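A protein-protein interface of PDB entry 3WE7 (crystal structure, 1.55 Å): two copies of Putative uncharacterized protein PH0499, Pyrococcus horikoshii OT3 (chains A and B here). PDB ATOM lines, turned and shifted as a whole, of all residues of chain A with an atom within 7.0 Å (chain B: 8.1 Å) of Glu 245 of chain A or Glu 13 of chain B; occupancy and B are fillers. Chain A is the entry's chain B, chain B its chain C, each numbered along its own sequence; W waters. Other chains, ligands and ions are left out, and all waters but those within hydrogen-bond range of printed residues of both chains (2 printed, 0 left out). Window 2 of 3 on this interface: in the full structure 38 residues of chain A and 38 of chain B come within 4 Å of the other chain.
Water W1 lies within hydrogen-bond range of the side-chain carboxylate (OE1) of Glu 13 of chain B (2.8 Å) and the side-chain carboxylate (OE2) of Glu 245 of chain A (3.0 Å). Water W2 lies within hydrogen-bond range of the backbone carbonyl oxygen (O) of Asp 10 of chain B (2.9 Å) and the guanidinium group (NH1) of Arg 250 of chain A (3.4 Å).
Printed residues of chain A that touch a printed residue of chain B: Met 241, Phe 242, Glu 245 and Arg 250. Hydrophobic or aromatic side chains of chain A that line the printed part of chain B: Met 241 and Phe 242. Along chain A the printed residues that touch a printed residue of chain B span positions 241 to 250. Of the 13 printed residues of chain B, 6 touch a printed residue of chain A. Hydrophobic or aromatic side chains of chain B within 4 Å of the printed part of chain A: Phe 12 and Ala 15. Among the printed residues, no Asp or Glu carboxylate lies within 4 Å of a Lys or Arg side-chain nitrogen of the other chain.
No position is printed for both chains. Of the 10 pairs that touch across the chains among the printed residues, none has its exchanged pair printed and touching as well.
O of Glu 13 of chain B sits at hydrogen-bond distance from ND2 of Asn 17 of chain B (3.2 Å). N of Glu 14 of chain B is in hydrogen-bond range of OG1 of Thr 11 of chain B. The side-chain hydroxyl (OH) of Tyr 251 of chain A is in hydrogen-bond range of the guanidinium group (NE) of Arg 250 of chain A. The backbone NH (N) of Glu 13 of chain B lies close to the side-chain hydroxyl (OG1) of Thr 11 of chain B, at 3.5 Å. The backbone NH (N) of Asp 10 of chain B lies close to the side-chain carboxylate (OE1) of Glu 14 of chain B (3.5 Å).
Met 241 of chain A touches Ile 9 of chain B. Met 241 of chain A touches Asp 10 of chain B (CE to O, 3.7 Å). Thr 11 of chain B touches Met 241 of chain A (C to CE, 3.5 Å). CE of Met 241 of chain A touches N of Phe 12 of chain B, at 3.7 Å. SD of Met 241 of chain A touches CB of Ala 15 of chain B (3.7 Å). CD1 of Phe 12 of chain B touches N of Phe 242 of chain A, at 3.4 Å. OE1 of Glu 245 of chain A touches CD2 of Phe 12 of chain B, 3.5 Å away. Asp 10 of chain B touches Arg 250 of chain A (O to NH1, 3.7 Å).
OE2 of Glu 245 of chain A sits close to OE2 of Glu 13 of chain B (2.5 Å). The guanidinium group (NH1) of Arg 250 of chain A is in hydrogen-bond range of the backbone carbonyl oxygen (O) of Ile 9 of chain B.
Glu 245 of chain A touches just these residues of chain B: Phe 12 and Glu 13. No residue of chain B comes within 4 Å of Gly 244 of chain A. Printed residues of chain A within 4 Å of Asp 10 of chain B: Met 241 (3.7 Å) and Arg 250 (3.7 Å). Printed residues of chain A within 4 Å of Ile 9 of chain B: Met 241 (3.7 Å) and Arg 250 (2.6 Å). Of the printed residues of chain B, Met 241 of chain A touches Ile 9 (3.7 Å), Asp 10 (3.7 Å), Thr 11 (3.5 Å), Phe 12 (3.7 Å) and Ala 15 (3.7 Å). Printed residues of chain A within 4 Å of Ala 15 of chain B: Met 241 (3.7 Å). The nearest printed residue of chain A that does not touch Ala 15 of chain B is Phe 242 of chain A (7.0 Å).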
ATOM      1  N   ILE A 203     -24.657   4.004  25.486  1.00  0.00           N
ATOM      2  CA  ILE A 203     -23.862   5.078  26.071  1.00  0.00           C
ATOM      3  C   ILE A 203     -23.447   4.682  27.457  1.00  0.00           C
ATOM      4  O   ILE A 203     -24.261   4.156  28.266  1.00  0.00           O
ATOM      5  CB  ILE A 203     -24.669   6.374  26.324  1.00  0.00           C
ATOM      6  CG1 ILE A 203     -25.468   6.825  25.094  1.00  0.00           C
ATOM      7  CG2 ILE A 203     -23.737   7.516  26.836  1.00  0.00           C
ATOM      8  CD1 ILE A 203     -24.593   7.251  23.930  1.00  0.00           C
ATOM      9  N   ALA A 240     -18.456  14.831  25.008  1.00  0.00           N
ATOM     10  CA  ALA A 240     -19.027  14.013  26.031  1.00  0.00           C
ATOM     11  C   ALA A 240     -20.466  14.397  26.390  1.00  0.00           C
ATOM     12  O   ALA A 240     -21.257  13.464  26.775  1.00  0.00           O
ATOM     13  CB  ALA A 240     -18.121  14.032  27.293  1.00  0.00           C
ATOM     14  N   MET A 241     -20.789  15.702  26.298  1.00  0.00           N
ATOM     15  CA  MET A 241     -22.170  16.082  26.586  1.00  0.00           C
ATOM     16  C   MET A 241     -23.117  15.614  25.490  1.00  0.00           C
ATOM     17  O   MET A 241     -24.294  15.244  25.803  1.00  0.00           O
ATOM     18  CB  MET A 241     -22.331  17.634  26.709  1.00  0.00           C
ATOM     19  CG  MET A 241     -21.545  18.101  27.940  1.00  0.00           C
ATOM     20  SD  MET A 241     -21.853  19.832  28.313  1.00  0.00           S
ATOM     21  CE  MET A 241     -23.345  19.684  29.220  1.00  0.00           C
ATOM     22  N   PHE A 242     -22.675  15.599  24.210  1.00  0.00           N
ATOM     23  CA  PHE A 242     -23.495  15.047  23.132  1.00  0.00           C
ATOM     24  C   PHE A 242     -23.925  13.612  23.447  1.00  0.00           C
ATOM     25  O   PHE A 242     -25.126  13.208  23.234  1.00  0.00           O
ATOM     26  CB  PHE A 242     -22.669  14.989  21.830  1.00  0.00           C
ATOM     27  CG  PHE A 242     -23.313  14.272  20.695  1.00  0.00           C
ATOM     28  CD1 PHE A 242     -22.839  13.003  20.361  1.00  0.00           C
ATOM     29  CD2 PHE A 242     -24.296  14.904  19.939  1.00  0.00           C
ATOM     30  CE1 PHE A 242     -23.379  12.321  19.292  1.00  0.00           C
ATOM     31  CE2 PHE A 242     -24.869  14.213  18.876  1.00  0.00           C
ATOM     32  CZ  PHE A 242     -24.408  12.955  18.564  1.00  0.00           C
ATOM     33  N   TYR A 243     -22.969  12.819  23.950  1.00  0.00           N
ATOM     34  CA  TYR A 243     -23.302  11.414  24.221  1.00  0.00           C
ATOM     35  C   TYR A 243     -24.119  11.324  25.506  1.00  0.00           C
ATOM     36  O   TYR A 243     -25.157  10.545  25.548  1.00  0.00           O
ATOM     37  CB  TYR A 243     -22.066  10.502  24.280  1.00  0.00           C
ATOM     38  CG  TYR A 243     -21.311  10.384  23.009  1.00  0.00           C
ATOM     39  CD1 TYR A 243     -21.925   9.920  21.866  1.00  0.00           C
ATOM     40  CD2 TYR A 243     -19.932  10.707  22.944  1.00  0.00           C
ATOM     41  CE1 TYR A 243     -21.224   9.716  20.716  1.00  0.00           C
ATOM     42  CE2 TYR A 243     -19.233  10.529  21.752  1.00  0.00           C
ATOM     43  CZ  TYR A 243     -19.878  10.124  20.621  1.00  0.00           C
ATOM     44  OH  TYR A 243     -19.223   9.936  19.428  1.00  0.00           O
ATOM     45  N   GLY A 244     -23.680  12.027  26.576  1.00  0.00           N
ATOM     46  CA  GLY A 244     -24.367  11.961  27.839  1.00  0.00           C
ATOM     47  C   GLY A 244     -25.859  12.273  27.814  1.00  0.00           C
ATOM     48  O   GLY A 244     -26.675  11.554  28.423  1.00  0.00           O
ATOM     49  N   GLU A 245     -26.210  13.274  27.020  1.00  0.00           N
ATOM     50  CA  GLU A 245     -27.559  13.804  27.000  1.00  0.00           C
ATOM     51  C   GLU A 245     -28.449  12.661  26.586  1.00  0.00           C
ATOM     52  O   GLU A 245     -29.630  12.620  27.053  1.00  0.00           O
ATOM     53  CB  GLU A 245     -27.637  14.827  25.845  1.00  0.00           C
ATOM     54  CG  GLU A 245     -29.095  15.405  25.738  1.00  0.00           C
ATOM     55  CD  GLU A 245     -29.233  16.491  24.683  1.00  0.00           C
ATOM     56  OE1 GLU A 245     -28.360  16.655  23.834  1.00  0.00           O
ATOM     57  OE2 GLU A 245     -30.297  17.206  24.667  1.00  0.00           O
ATOM     58  N   LYS A 246     -27.975  11.795  25.663  1.00  0.00           N
ATOM     59  CA  LYS A 246     -28.750  10.640  25.208  1.00  0.00           C
ATOM     60  C   LYS A 246     -29.232   9.654  26.257  1.00  0.00           C
ATOM     61  O   LYS A 246     -30.177   8.849  26.008  1.00  0.00           O
ATOM     62  CB  LYS A 246     -28.003   9.857  24.100  1.00  0.00           C
ATOM     63  CG  LYS A 246     -27.778  10.788  22.909  1.00  0.00           C
ATOM     64  CD  LYS A 246     -26.961  10.160  21.759  1.00  0.00           C
ATOM     65  CE  LYS A 246     -26.832  11.109  20.580  1.00  0.00           C
ATOM     66  NZ  LYS A 246     -28.179  11.305  19.936  1.00  0.00           N
ATOM     67  N   ILE A 247     -28.617   9.653  27.427  1.00  0.00           N
ATOM     68  CA  ILE A 247     -29.130   8.820  28.549  1.00  0.00           C
ATOM     69  C   ILE A 247     -29.402   9.683  29.821  1.00  0.00           C
ATOM     70  O   ILE A 247     -29.376   9.210  30.970  1.00  0.00           O
ATOM     71  CB  ILE A 247     -28.211   7.654  28.880  1.00  0.00           C
ATOM     72  CG1 ILE A 247     -26.742   8.120  29.164  1.00  0.00           C
ATOM     73  CG2 ILE A 247     -28.259   6.671  27.685  1.00  0.00           C
ATOM     74  CD1 ILE A 247     -25.836   7.098  29.909  1.00  0.00           C
ATOM     75  N   GLY A 248     -29.488  10.997  29.581  1.00  0.00           N
ATOM     76  CA  GLY A 248     -29.863  11.899  30.664  1.00  0.00           C
ATOM     77  C   GLY A 248     -28.792  12.171  31.660  1.00  0.00           C
ATOM     78  O   GLY A 248     -29.108  12.496  32.757  1.00  0.00           O
ATOM     79  N   VAL A 249     -27.515  12.117  31.236  1.00  0.00           N
ATOM     80  CA  VAL A 249     -26.408  12.398  32.163  1.00  0.00           C
ATOM     81  C   VAL A 249     -25.521  13.460  31.555  1.00  0.00           C
ATOM     82  O   VAL A 249     -25.631  13.819  30.383  1.00  0.00           O
ATOM     83  CB  VAL A 249     -25.597  11.118  32.499  1.00  0.00           C
ATOM     84  CG1 VAL A 249     -26.503   9.962  33.031  1.00  0.00           C
ATOM     85  CG2 VAL A 249     -24.740  10.664  31.282  1.00  0.00           C
ATOM     86  N   ARG A 250     -24.676  14.013  32.387  1.00  0.00           N
ATOM     87  CA  ARG A 250     -23.930  15.151  31.898  1.00  0.00           C
ATOM     88  C   ARG A 250     -22.874  14.764  30.852  1.00  0.00           C
ATOM     89  O   ARG A 250     -22.781  15.400  29.771  1.00  0.00           O
ATOM     90  CB  ARG A 250     -23.229  15.846  33.064  1.00  0.00           C
ATOM     91  CG  ARG A 250     -22.525  17.124  32.635  1.00  0.00           C
ATOM     92  CD  ARG A 250     -21.968  17.791  33.916  1.00  0.00           C
ATOM     93  NE  ARG A 250     -21.218  18.980  33.599  1.00  0.00           N
ATOM     94  CZ  ARG A 250     -21.743  20.091  33.082  1.00  0.00           C
ATOM     95  NH1 ARG A 250     -23.045  20.182  32.768  1.00  0.00           N
ATOM     96  NH2 ARG A 250     -20.952  21.091  32.808  1.00  0.00           N
ATOM     97  N   TYR A 251     -22.102  13.744  31.108  1.00  0.00           N
ATOM     98  CA  TYR A 251     -21.035  13.336  30.167  1.00  0.00           C
ATOM     99  C   TYR A 251     -21.115  11.821  29.938  1.00  0.00           C
ATOM    100  O   TYR A 251     -21.251  10.977  30.901  1.00  0.00           O
ATOM    101  CB  TYR A 251     -19.674  13.582  30.846  1.00  0.00           C
ATOM    102  CG  TYR A 251     -19.376  15.022  31.100  1.00  0.00           C
ATOM    103  CD1 TYR A 251     -19.403  15.959  30.089  1.00  0.00           C
ATOM    104  CD2 TYR A 251     -18.943  15.407  32.395  1.00  0.00           C
ATOM    105  CE1 TYR A 251     -19.032  17.317  30.372  1.00  0.00           C
ATOM    106  CE2 TYR A 251     -18.524  16.754  32.664  1.00  0.00           C
ATOM    107  CZ  TYR A 251     -18.607  17.657  31.630  1.00  0.00           C
ATOM    108  OH  TYR A 251     -18.280  19.014  31.846  1.00  0.00           O
ATOM    109  N   GLY A 252     -20.968  11.450  28.683  1.00  0.00           N
ATOM    110  CA  GLY A 252     -21.028   9.975  28.308  1.00  0.00           C
ATOM    111  C   GLY A 252     -19.979   9.677  27.236  1.00  0.00           C
ATOM    112  O   GLY A 252     -19.407  10.594  26.620  1.00  0.00           O
ATOM    113  N   ILE B   9     -21.356  24.606  32.149  1.00  0.00           N
ATOM    114  CA  ILE B   9     -22.462  24.752  31.217  1.00  0.00           C
ATOM    115  C   ILE B   9     -23.428  23.625  31.414  1.00  0.00           C
ATOM    116  O   ILE B   9     -23.007  22.489  31.641  1.00  0.00           O
ATOM    117  CB  ILE B   9     -21.908  24.730  29.792  1.00  0.00           C
ATOM    118  CG1 ILE B   9     -21.020  25.955  29.628  1.00  0.00           C
ATOM    119  CG2 ILE B   9     -23.061  24.769  28.796  1.00  0.00           C
ATOM    120  CD1 ILE B   9     -20.217  25.965  28.357  1.00  0.00           C
ATOM    121  N   ASP B  10     -24.726  23.921  31.341  1.00  0.00           N
ATOM    122  CA  ASP B  10     -25.736  22.967  31.770  1.00  0.00           C
ATOM    123  C   ASP B  10     -26.101  21.888  30.744  1.00  0.00           C
ATOM    124  O   ASP B  10     -26.344  20.786  31.156  1.00  0.00           O
ATOM    125  CB  ASP B  10     -27.025  23.689  32.197  1.00  0.00           C
ATOM    126  CG  ASP B  10     -26.868  24.421  33.524  1.00  0.00           C
ATOM    127  OD1 ASP B  10     -25.886  24.155  34.287  1.00  0.00           O
ATOM    128  OD2 ASP B  10     -27.743  25.277  33.800  1.00  0.00           O
ATOM    129  N   THR B  11     -26.202  22.241  29.452  1.00  0.00           N
ATOM    130  CA  THR B  11     -26.747  21.320  28.424  1.00  0.00           C
ATOM    131  C   THR B  11     -25.756  21.225  27.261  1.00  0.00           C
ATOM    132  O   THR B  11     -24.872  22.147  27.088  1.00  0.00           O
ATOM    133  CB  THR B  11     -28.128  21.706  27.861  1.00  0.00           C
ATOM    134  OG1 THR B  11     -28.037  22.916  27.088  1.00  0.00           O
ATOM    135  CG2 THR B  11     -29.202  21.830  29.019  1.00  0.00           C
ATOM    136  N   PHE B  12     -25.870  20.116  26.552  1.00  0.00           N
ATOM    137  CA  PHE B  12     -25.150  19.930  25.295  1.00  0.00           C
ATOM    138  C   PHE B  12     -25.456  21.067  24.351  1.00  0.00           C
ATOM    139  O   PHE B  12     -24.524  21.632  23.728  1.00  0.00           O
ATOM    140  CB  PHE B  12     -25.478  18.587  24.645  1.00  0.00           C
ATOM    141  CG  PHE B  12     -25.015  18.545  23.239  1.00  0.00           C
ATOM    142  CD1 PHE B  12     -23.651  18.576  22.892  1.00  0.00           C
ATOM    143  CD2 PHE B  12     -25.945  18.651  22.228  1.00  0.00           C
ATOM    144  CE1 PHE B  12     -23.266  18.621  21.560  1.00  0.00           C
ATOM    145  CE2 PHE B  12     -25.574  18.663  20.888  1.00  0.00           C
ATOM    146  CZ  PHE B  12     -24.209  18.656  20.527  1.00  0.00           C
ATOM    147  N   GLU B  13     -26.740  21.420  24.216  1.00  0.00           N
ATOM    148  CA  GLU B  13     -27.048  22.505  23.246  1.00  0.00           C
ATOM    149  C   GLU B  13     -26.296  23.809  23.603  1.00  0.00           C
ATOM    150  O   GLU B  13     -25.747  24.476  22.711  1.00  0.00           O
ATOM    151  CB  GLU B  13     -28.583  22.692  23.141  1.00  0.00           C
ATOM    152  CG  GLU B  13     -29.320  21.421  22.634  1.00  0.00           C
ATOM    153  CD  GLU B  13     -29.627  20.326  23.684  1.00  0.00           C
ATOM    154  OE1 GLU B  13     -29.303  20.454  24.913  1.00  0.00           O
ATOM    155  OE2 GLU B  13     -30.205  19.282  23.207  1.00  0.00           O
ATOM    156  N   GLU B  14     -26.255  24.178  24.886  1.00  0.00           N
ATOM    157  CA  GLU B  14     -25.461  25.319  25.324  1.00  0.00           C
ATOM    158  C   GLU B  14     -23.989  25.171  25.057  1.00  0.00           C
ATOM    159  O   GLU B  14     -23.383  26.096  24.538  1.00  0.00           O
ATOM    160  CB  GLU B  14     -25.705  25.671  26.788  1.00  0.00           C
ATOM    161  CG  GLU B  14     -27.204  25.972  26.934  1.00  0.00           C
ATOM    162  CD  GLU B  14     -27.660  26.097  28.378  1.00  0.00           C
ATOM    163  OE1 GLU B  14     -27.111  25.424  29.291  1.00  0.00           O
ATOM    164  OE2 GLU B  14     -28.565  26.921  28.587  1.00  0.00           O
ATOM    165  N   ALA B  15     -23.412  24.010  25.358  1.00  0.00           N
ATOM    166  CA  ALA B  15     -21.989  23.769  25.106  1.00  0.00           C
ATOM    167  C   ALA B  15     -21.651  23.834  23.649  1.00  0.00           C
ATOM    168  O   ALA B  15     -20.635  24.450  23.282  1.00  0.00           O
ATOM    169  CB  ALA B  15     -21.725  22.354  25.642  1.00  0.00           C
ATOM    170  N   PHE B  16     -22.497  23.247  22.795  1.00  0.00           N
ATOM    171  CA  PHE B  16     -22.226  23.278  21.353  1.00  0.00           C
ATOM    172  C   PHE B  16     -22.145  24.726  20.834  1.00  0.00           C
ATOM    173  O   PHE B  16     -21.194  25.109  20.123  1.00  0.00           O
ATOM    174  CB  PHE B  16     -23.273  22.555  20.591  1.00  0.00           C
ATOM    175  CG  PHE B  16     -23.036  22.591  19.145  1.00  0.00           C
ATOM    176  CD1 PHE B  16     -22.055  21.778  18.552  1.00  0.00           C
ATOM    177  CD2 PHE B  16     -23.757  23.503  18.336  1.00  0.00           C
ATOM    178  CE1 PHE B  16     -21.869  21.841  17.160  1.00  0.00           C
ATOM    179  CE2 PHE B  16     -23.503  23.613  16.985  1.00  0.00           C
ATOM    180  CZ  PHE B  16     -22.567  22.752  16.386  1.00  0.00           C
ATOM    181  N   ASN B  17     -23.133  25.544  21.239  1.00  0.00           N
ATOM    182  CA  ASN B  17     -23.094  26.939  20.793  1.00  0.00           C
ATOM    183  C   ASN B  17     -21.916  27.715  21.319  1.00  0.00           C
ATOM    184  O   ASN B  17     -21.315  28.441  20.573  1.00  0.00           O
ATOM    185  CB  ASN B  17     -24.486  27.594  21.019  1.00  0.00           C
ATOM    186  CG  ASN B  17     -25.471  27.095  20.016  1.00  0.00           C
ATOM    187  OD1 ASN B  17     -25.223  27.125  18.828  1.00  0.00           O
ATOM    188  ND2 ASN B  17     -26.572  26.575  20.473  1.00  0.00           N
ATOM    189  N   LYS B  18     -21.508  27.530  22.597  1.00  0.00           N
ATOM    190  CA  LYS B  18     -20.347  28.175  23.122  1.00  0.00           C
ATOM    191  C   LYS B  18     -19.038  27.716  22.427  1.00  0.00           C
ATOM    192  O   LYS B  18     -18.129  28.502  22.086  1.00  0.00           O
ATOM    193  CB  LYS B  18     -20.308  27.942  24.645  1.00  0.00           C
ATOM    194  CG  LYS B  18     -19.730  29.089  25.470  1.00  0.00           C
ATOM    195  CD  LYS B  18     -20.613  29.277  26.730  1.00  0.00           C
ATOM    196  CE  LYS B  18     -20.453  30.616  27.458  1.00  0.00           C
ATOM    197  NZ  LYS B  18     -21.384  31.680  26.982  1.00  0.00           N
ATOM    198  N   LEU B  19     -18.900  26.400  22.256  1.00  0.00           N
ATOM    199  CA  LEU B  19     -17.790  25.856  21.506  1.00  0.00           C
ATOM    200  C   LEU B  19     -17.700  26.432  20.108  1.00  0.00           C
ATOM    201  O   LEU B  19     -16.600  26.852  19.716  1.00  0.00           O
ATOM    202  CB  LEU B  19     -17.941  24.303  21.432  1.00  0.00           C
ATOM    203  CG  LEU B  19     -16.802  23.654  20.639  1.00  0.00           C
ATOM    204  CD1 LEU B  19     -15.413  23.640  21.395  1.00  0.00           C
ATOM    205  CD2 LEU B  19     -17.337  22.249  20.292  1.00  0.00           C
ATOM    206  N   LEU B  20     -18.779  26.441  19.385  1.00  0.00           N
ATOM    207  CA  LEU B  20     -18.710  26.832  17.962  1.00  0.00           C
ATOM    208  C   LEU B  20     -18.434  28.302  17.879  1.00  0.00           C
ATOM    209  O   LEU B  20     -17.562  28.720  17.078  1.00  0.00           O
ATOM    210  CB  LEU B  20     -20.051  26.573  17.295  1.00  0.00           C
ATOM    211  CG  LEU B  20     -20.094  26.741  15.793  1.00  0.00           C
ATOM    212  CD1 LEU B  20     -19.118  25.740  15.091  1.00  0.00           C
ATOM    213  CD2 LEU B  20     -21.541  26.650  15.197  1.00  0.00           C
ATOM    214  N   LEU B 271     -24.757  19.475  12.589  1.00  0.00           N
ATOM    215  CA  LEU B 271     -25.380  20.674  13.167  1.00  0.00           C
ATOM    216  C   LEU B 271     -24.904  21.921  12.488  1.00  0.00           C
ATOM    217  O   LEU B 271     -25.349  23.029  12.839  1.00  0.00           O
ATOM    218  CB  LEU B 271     -25.022  20.737  14.634  1.00  0.00           C
ATOM    219  CG  LEU B 271     -25.694  19.619  15.489  1.00  0.00           C
ATOM    220  CD1 LEU B 271     -25.273  19.852  16.926  1.00  0.00           C
ATOM    221  CD2 LEU B 271     -27.228  19.521  15.297  1.00  0.00           C
HETATM  222  O   HOH W   1     -30.909  19.152  26.856  1.00  0.00           O
HETATM  223  O   HOH W   2     -25.826  18.285  32.524  1.00  0.00           O
